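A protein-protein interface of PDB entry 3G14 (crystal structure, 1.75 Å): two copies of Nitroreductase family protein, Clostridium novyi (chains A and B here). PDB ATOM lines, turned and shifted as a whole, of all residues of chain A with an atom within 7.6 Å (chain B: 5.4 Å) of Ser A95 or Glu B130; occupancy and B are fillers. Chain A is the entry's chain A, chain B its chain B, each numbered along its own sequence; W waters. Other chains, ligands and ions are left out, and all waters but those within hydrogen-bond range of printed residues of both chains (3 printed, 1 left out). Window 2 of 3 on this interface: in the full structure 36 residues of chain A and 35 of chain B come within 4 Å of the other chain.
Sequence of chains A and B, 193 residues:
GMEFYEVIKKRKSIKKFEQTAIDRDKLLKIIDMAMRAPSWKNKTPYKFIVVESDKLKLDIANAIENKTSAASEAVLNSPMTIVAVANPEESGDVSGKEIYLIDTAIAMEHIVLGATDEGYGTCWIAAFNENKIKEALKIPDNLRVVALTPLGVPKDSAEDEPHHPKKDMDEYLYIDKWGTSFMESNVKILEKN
The side-chain hydroxyl (OG) of Ser A95 lies within hydrogen-bond range of the backbone carbonyl oxygen (O) of Phe B128 (2.8 Å). The backbone carbonyl oxygen of Ser A95 is in hydrogen-bond range of the guanidinium group of Arg B144, at 3.1 Å. O of Gly A96 lies within hydrogen-bond range of NH2 of Arg B144, at 3.3 Å. O of Ala B126 sits at hydrogen-bond distance from NZ of Lys A97 (2.7 Å). The side-chain amino group of Lys A97 lies within hydrogen-bond range of the backbone carbonyl oxygen of Val B145 (3.3 Å).
The backbone carbonyl oxygen of Ala B127 lies within hydrogen-bond range of the backbone NH of Glu B65, at 3.0 Å. The side-chain carboxylate (OE2) of Glu B130 is in salt-bridge range of the guanidinium group (NE) of Arg B144, at 3.0 Å. The backbone NH (N) of Val B145 lies within hydrogen-bond range of the side-chain carboxylate (OE2) of Glu B130.
Among the printed residues, merely in contact across the chains: Val A94 with Ala B126 (3.8 Å), Val A94 with Ala B127 (3.7 Å), Ser A95 with Ala B126 (3.8 Å), Ser A95 with Ala B127 (3.7 Å), Ser A95 with Glu B130 (3.7 Å), Lys A97 with Phe B128 (3.3 Å) and Lys A97 with Arg B144 (3.96 Å).
Ser A95 touches five residues of chain B. Printed residues of chain B within 4 Å of Lys A97: Ala B126, Phe B128, Arg B144 and Val B145. Of the printed residues of chain A, Phe B128 touches Ser A95 (2.8 Å) and Lys A97 (3.3 Å). Of chain A, only Ser A95 (3.7 Å) comes within 4 Å of Glu B130.
Of the 14 printed residues of chain B, 6 touch a printed residue of chain A. Hydrophobic or aromatic side chains of chain B that line the printed part of chain A: Ala B127 and Phe B128. Among the printed residues, no Asp or Glu carboxylate lies within 4 Å of a Lys or Arg side-chain nitrogen of the other chain.
No position is printed for both chains. Of the 12 pairs that touch across the chains among the printed residues, none has its exchanged pair printed and touching as well.
Water W2 lies within hydrogen-bond range of the side-chain carboxylate (OE1) of Glu B65 (2.6 Å), the backbone carbonyl oxygen (O) of Phe B128 (3.1 Å) and the side-chain hydroxyl (OG) of Ser A95 (3.3 Å). Water W3 lies within hydrogen-bond range of the side-chain carboxylate of Glu B65 and the side-chain hydroxyl of Ser A95. Water W1 bridges the side-chain carboxylate (OE1) of Glu B130 (2.8 Å) and the backbone carbonyl oxygen (O) of Ser A95 (3.1 Å).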
ATOM      1  N   ASP A  93     -22.604  -8.494 -18.887  1.00  0.00           N
ATOM      2  CA  ASP A  93     -22.205  -7.100 -18.857  1.00  0.00           C
ATOM      3  C   ASP A  93     -23.397  -6.183 -18.905  1.00  0.00           C
ATOM      4  O   ASP A  93     -24.423  -6.513 -19.536  1.00  0.00           O
ATOM      5  CB  ASP A  93     -21.333  -6.786 -20.038  1.00  0.00           C
ATOM      6  CG  ASP A  93     -20.052  -7.524 -20.021  1.00  0.00           C
ATOM      7  OD1 ASP A  93     -19.658  -8.045 -18.954  1.00  0.00           O
ATOM      8  OD2 ASP A  93     -19.441  -7.561 -21.107  1.00  0.00           O
ATOM      9  N   VAL A  94     -23.255  -5.033 -18.239  1.00  0.00           N
ATOM     10  CA  VAL A  94     -24.285  -4.007 -18.198  1.00  0.00           C
ATOM     11  C   VAL A  94     -23.584  -2.684 -18.524  1.00  0.00           C
ATOM     12  O   VAL A  94     -22.617  -2.339 -17.855  1.00  0.00           O
ATOM     13  CB  VAL A  94     -24.936  -3.949 -16.778  1.00  0.00           C
ATOM     14  CG1 VAL A  94     -25.984  -2.906 -16.695  1.00  0.00           C
ATOM     15  CG2 VAL A  94     -25.522  -5.352 -16.410  1.00  0.00           C
ATOM     16  N   SER A  95     -24.063  -1.990 -19.547  1.00  0.00           N
ATOM     17  CA  SER A  95     -23.517  -0.687 -19.984  1.00  0.00           C
ATOM     18  C   SER A  95     -21.964  -0.676 -20.087  1.00  0.00           C
ATOM     19  O   SER A  95     -21.262   0.259 -19.623  1.00  0.00           O
ATOM     20  CB  SER A  95     -24.074   0.430 -19.089  1.00  0.00           C
ATOM     21  OG  SER A  95     -25.477   0.547 -19.283  1.00  0.00           O
ATOM     22  N   GLY A  96     -21.438  -1.729 -20.713  1.00  0.00           N
ATOM     23  CA  GLY A  96     -20.005  -1.822 -21.011  1.00  0.00           C
ATOM     24  C   GLY A  96     -19.150  -2.215 -19.818  1.00  0.00           C
ATOM     25  O   GLY A  96     -17.929  -1.984 -19.831  1.00  0.00           O
ATOM     26  N   LYS A  97     -19.782  -2.792 -18.794  1.00  0.00           N
ATOM     27  CA  LYS A  97     -19.132  -3.102 -17.518  1.00  0.00           C
ATOM     28  C   LYS A  97     -19.423  -4.545 -17.105  1.00  0.00           C
ATOM     29  O   LYS A  97     -20.562  -5.010 -17.192  1.00  0.00           O
ATOM     30  CB  LYS A  97     -19.607  -2.197 -16.372  1.00  0.00           C
ATOM     31  CG  LYS A  97     -19.331  -0.703 -16.560  1.00  0.00           C
ATOM     32  CD  LYS A  97     -20.121   0.167 -15.589  1.00  0.00           C
ATOM     33  CE  LYS A  97     -21.652  -0.007 -15.779  1.00  0.00           C
ATOM     34  NZ  LYS A  97     -22.434   1.243 -15.557  1.00  0.00           N
ATOM     35  N   GLU A  98     -18.392  -5.239 -16.626  1.00  0.00           N
ATOM     36  CA  GLU A  98     -18.559  -6.598 -16.129  1.00  0.00           C
ATOM     37  C   GLU A  98     -19.182  -6.584 -14.757  1.00  0.00           C
ATOM     38  O   GLU A  98     -18.527  -6.276 -13.756  1.00  0.00           O
ATOM     39  CB  GLU A  98     -17.229  -7.330 -16.077  1.00  0.00           C
ATOM     40  CG  GLU A  98     -16.625  -7.543 -17.466  1.00  0.00           C
ATOM     41  CD  GLU A  98     -15.581  -6.485 -17.813  1.00  0.00           C
ATOM     42  OE1 GLU A  98     -15.787  -5.267 -17.538  1.00  0.00           O
ATOM     43  OE2 GLU A  98     -14.547  -6.884 -18.381  1.00  0.00           O
ATOM     44  N   ILE A  99     -20.472  -6.908 -14.731  1.00  0.00           N
ATOM     45  CA  ILE A  99     -21.247  -6.925 -13.496  1.00  0.00           C
ATOM     46  C   ILE A  99     -20.632  -7.756 -12.405  1.00  0.00           C
ATOM     47  O   ILE A  99     -20.682  -7.379 -11.243  1.00  0.00           O
ATOM     48  CB  ILE A  99     -22.713  -7.342 -13.755  1.00  0.00           C
ATOM     49  CG1 ILE A  99     -23.494  -6.092 -14.129  1.00  0.00           C
ATOM     50  CG2 ILE A  99     -23.370  -8.055 -12.525  1.00  0.00           C
ATOM     51  CD1 ILE A  99     -23.339  -4.875 -13.155  1.00  0.00           C
ATOM     52  N   GLU B  65     -31.719   2.835 -18.130  1.00  0.00           N
ATOM     53  CA  GLU B  65     -32.215   1.792 -19.032  1.00  0.00           C
ATOM     54  C   GLU B  65     -32.713   0.547 -18.283  1.00  0.00           C
ATOM     55  O   GLU B  65     -32.141  -0.516 -18.395  1.00  0.00           O
ATOM     56  CB  GLU B  65     -31.131   1.429 -20.027  1.00  0.00           C
ATOM     57  CG  GLU B  65     -30.840   2.549 -21.017  1.00  0.00           C
ATOM     58  CD  GLU B  65     -29.615   2.315 -21.892  1.00  0.00           C
ATOM     59  OE1 GLU B  65     -28.725   1.495 -21.535  1.00  0.00           O
ATOM     60  OE2 GLU B  65     -29.556   3.005 -22.930  1.00  0.00           O
ATOM     61  N   ALA B 126     -26.801   0.820 -12.275  1.00  0.00           N
ATOM     62  CA  ALA B 126     -25.651   0.555 -13.113  1.00  0.00           C
ATOM     63  C   ALA B 126     -25.989   0.540 -14.613  1.00  0.00           C
ATOM     64  O   ALA B 126     -25.071   0.540 -15.440  1.00  0.00           O
ATOM     65  CB  ALA B 126     -25.024  -0.766 -12.750  1.00  0.00           C
ATOM     66  N   ALA B 127     -27.287   0.509 -14.942  1.00  0.00           N
ATOM     67  CA  ALA B 127     -27.758   0.391 -16.351  1.00  0.00           C
ATOM     68  C   ALA B 127     -28.286   1.727 -16.882  1.00  0.00           C
ATOM     69  O   ALA B 127     -29.340   2.200 -16.466  1.00  0.00           O
ATOM     70  CB  ALA B 127     -28.860  -0.666 -16.465  1.00  0.00           C
ATOM     71  N   PHE B 128     -27.542   2.319 -17.813  1.00  0.00           N
ATOM     72  CA  PHE B 128     -27.876   3.629 -18.349  1.00  0.00           C
ATOM     73  C   PHE B 128     -27.139   3.828 -19.656  1.00  0.00           C
ATOM     74  O   PHE B 128     -26.147   3.139 -19.953  1.00  0.00           O
ATOM     75  CB  PHE B 128     -27.548   4.774 -17.369  1.00  0.00           C
ATOM     76  CG  PHE B 128     -26.284   4.551 -16.544  1.00  0.00           C
ATOM     77  CD1 PHE B 128     -25.020   4.574 -17.139  1.00  0.00           C
ATOM     78  CD2 PHE B 128     -26.379   4.324 -15.181  1.00  0.00           C
ATOM     79  CE1 PHE B 128     -23.857   4.358 -16.372  1.00  0.00           C
ATOM     80  CE2 PHE B 128     -25.243   4.108 -14.406  1.00  0.00           C
ATOM     81  CZ  PHE B 128     -23.984   4.132 -15.004  1.00  0.00           C
ATOM     82  N   ASN B 129     -27.664   4.743 -20.441  1.00  0.00           N
ATOM     83  CA  ASN B 129     -26.959   5.313 -21.600  1.00  0.00           C
ATOM     84  C   ASN B 129     -25.840   6.207 -21.051  1.00  0.00           C
ATOM     85  O   ASN B 129     -26.042   7.353 -20.634  1.00  0.00           O
ATOM     86  CB  ASN B 129     -27.907   6.087 -22.471  1.00  0.00           C
ATOM     87  CG  ASN B 129     -27.242   6.658 -23.720  1.00  0.00           C
ATOM     88  OD1 ASN B 129     -26.051   6.990 -23.733  1.00  0.00           O
ATOM     89  ND2 ASN B 129     -28.011   6.753 -24.783  1.00  0.00           N
ATOM     90  N   GLU B 130     -24.653   5.624 -21.000  1.00  0.00           N
ATOM     91  CA  GLU B 130     -23.530   6.292 -20.405  1.00  0.00           C
ATOM     92  C   GLU B 130     -23.177   7.604 -21.132  1.00  0.00           C
ATOM     93  O   GLU B 130     -22.773   8.577 -20.501  1.00  0.00           O
ATOM     94  CB  GLU B 130     -22.335   5.334 -20.436  1.00  0.00           C
ATOM     95  CG  GLU B 130     -21.111   5.862 -19.767  1.00  0.00           C
ATOM     96  CD  GLU B 130     -20.002   4.823 -19.670  1.00  0.00           C
ATOM     97  OE1 GLU B 130     -20.121   3.735 -20.265  1.00  0.00           O
ATOM     98  OE2 GLU B 130     -18.988   5.121 -19.032  1.00  0.00           O
ATOM     99  N   ASN B 131     -23.292   7.618 -22.465  1.00  0.00           N
ATOM    100  CA  ASN B 131     -22.958   8.821 -23.211  1.00  0.00           C
ATOM    101  C   ASN B 131     -23.829   9.991 -22.814  1.00  0.00           C
ATOM    102  O   ASN B 131     -23.359  11.145 -22.731  1.00  0.00           O
ATOM    103  CB  ASN B 131     -23.102   8.578 -24.708  1.00  0.00           C
ATOM    104  CG  ASN B 131     -22.006   7.695 -25.265  1.00  0.00           C
ATOM    105  OD1 ASN B 131     -20.915   7.573 -24.700  1.00  0.00           O
ATOM    106  ND2 ASN B 131     -22.277   7.112 -26.410  1.00  0.00           N
ATOM    107  N   LYS B 132     -25.105   9.693 -22.577  1.00  0.00           N
ATOM    108  CA  LYS B 132     -26.043  10.716 -22.180  1.00  0.00           C
ATOM    109  C   LYS B 132     -25.701  11.259 -20.810  1.00  0.00           C
ATOM    110  O   LYS B 132     -25.837  12.474 -20.592  1.00  0.00           O
ATOM    111  CB  LYS B 132     -27.504  10.234 -22.259  1.00  0.00           C
ATOM    112  CG  LYS B 132     -28.031  10.242 -23.701  1.00  0.00           C
ATOM    113  CD  LYS B 132     -28.316  11.681 -24.183  1.00  0.00           C
ATOM    114  CE  LYS B 132     -28.090  11.893 -25.688  1.00  0.00           C
ATOM    115  NZ  LYS B 132     -28.347  13.340 -26.089  1.00  0.00           N
ATOM    116  N   ILE B 133     -25.253  10.407 -19.896  1.00  0.00           N
ATOM    117  CA  ILE B 133     -24.859  10.920 -18.572  1.00  0.00           C
ATOM    118  C   ILE B 133     -23.568  11.754 -18.680  1.00  0.00           C
ATOM    119  O   ILE B 133     -23.435  12.821 -18.068  1.00  0.00           O
ATOM    120  CB  ILE B 133     -24.739   9.816 -17.506  1.00  0.00           C
ATOM    121  CG1 ILE B 133     -26.155   9.237 -17.228  1.00  0.00           C
ATOM    122  CG2 ILE B 133     -24.069  10.405 -16.198  1.00  0.00           C
ATOM    123  CD1 ILE B 133     -26.209   8.090 -16.245  1.00  0.00           C
ATOM    124  N   LYS B 134     -22.633  11.322 -19.530  1.00  0.00           N
ATOM    125  CA  LYS B 134     -21.422  12.117 -19.735  1.00  0.00           C
ATOM    126  C   LYS B 134     -21.721  13.479 -20.323  1.00  0.00           C
ATOM    127  O   LYS B 134     -21.105  14.472 -19.933  1.00  0.00           O
ATOM    128  CB  LYS B 134     -20.452  11.398 -20.647  1.00  0.00           C
ATOM    129  CG  LYS B 134     -19.806  10.183 -20.014  1.00  0.00           C
ATOM    130  CD  LYS B 134     -19.001   9.496 -21.105  1.00  0.00           C
ATOM    131  CE  LYS B 134     -18.065   8.440 -20.581  1.00  0.00           C
ATOM    132  NZ  LYS B 134     -17.402   7.705 -21.703  1.00  0.00           N
ATOM    133  N   GLU B 135     -22.648  13.531 -21.278  1.00  0.00           N
ATOM    134  CA  GLU B 135     -23.079  14.801 -21.855  1.00  0.00           C
ATOM    135  C   GLU B 135     -23.763  15.716 -20.823  1.00  0.00           C
ATOM    136  O   GLU B 135     -23.520  16.921 -20.800  1.00  0.00           O
ATOM    137  CB  GLU B 135     -23.982  14.554 -23.075  1.00  0.00           C
ATOM    138  CG  GLU B 135     -23.222  13.931 -24.247  1.00  0.00           C
ATOM    139  CD  GLU B 135     -24.115  13.414 -25.387  1.00  0.00           C
ATOM    140  OE1 GLU B 135     -25.328  13.665 -25.369  1.00  0.00           O
ATOM    141  OE2 GLU B 135     -23.578  12.756 -26.314  1.00  0.00           O
ATOM    142  N   LEU B 143     -13.358   8.743 -19.691  1.00  0.00           N
ATOM    143  CA  LEU B 143     -13.688   8.201 -18.386  1.00  0.00           C
ATOM    144  C   LEU B 143     -14.930   7.321 -18.473  1.00  0.00           C
ATOM    145  O   LEU B 143     -15.602   7.309 -19.497  1.00  0.00           O
ATOM    146  CB  LEU B 143     -13.906   9.345 -17.409  1.00  0.00           C
ATOM    147  CG  LEU B 143     -12.688  10.280 -17.278  1.00  0.00           C
ATOM    148  CD1 LEU B 143     -13.029  11.497 -16.415  1.00  0.00           C
ATOM    149  CD2 LEU B 143     -11.489   9.556 -16.700  1.00  0.00           C
ATOM    150  N   ARG B 144     -15.233   6.599 -17.387  1.00  0.00           N
ATOM    151  CA  ARG B 144     -16.354   5.659 -17.344  1.00  0.00           C
ATOM    152  C   ARG B 144     -17.276   6.039 -16.201  1.00  0.00           C
ATOM    153  O   ARG B 144     -16.800   6.347 -15.112  1.00  0.00           O
ATOM    154  CB  ARG B 144     -15.872   4.205 -17.187  1.00  0.00           C
ATOM    155  CG  ARG B 144     -14.944   3.727 -18.324  1.00  0.00           C
ATOM    156  CD  ARG B 144     -15.594   3.763 -19.709  1.00  0.00           C
ATOM    157  NE  ARG B 144     -16.902   3.093 -19.737  1.00  0.00           N
ATOM    158  CZ  ARG B 144     -17.101   1.776 -19.814  1.00  0.00           C
ATOM    159  NH1 ARG B 144     -16.091   0.930 -19.891  1.00  0.00           N
ATOM    160  NH2 ARG B 144     -18.340   1.304 -19.828  1.00  0.00           N
ATOM    161  N   VAL B 145     -18.581   6.052 -16.471  1.00  0.00           N
ATOM    162  CA  VAL B 145     -19.597   6.180 -15.416  1.00  0.00           C
ATOM    163  C   VAL B 145     -19.879   4.770 -14.881  1.00  0.00           C
ATOM    164  O   VAL B 145     -20.477   3.940 -15.561  1.00  0.00           O
ATOM    165  CB  VAL B 145     -20.892   6.918 -15.896  1.00  0.00           C
ATOM    166  CG1 VAL B 145     -21.903   7.086 -14.725  1.00  0.00           C
ATOM    167  CG2 VAL B 145     -20.513   8.281 -16.566  1.00  0.00           C
HETATM  168  O   HOH W   1     -21.539   2.151 -22.091  1.00  0.00           O
HETATM  169  O   HOH W   2     -26.251   1.172 -22.396  1.00  0.00           O
HETATM  170  O   HOH W   3     -28.144  -0.829 -20.211  1.00  0.00           O
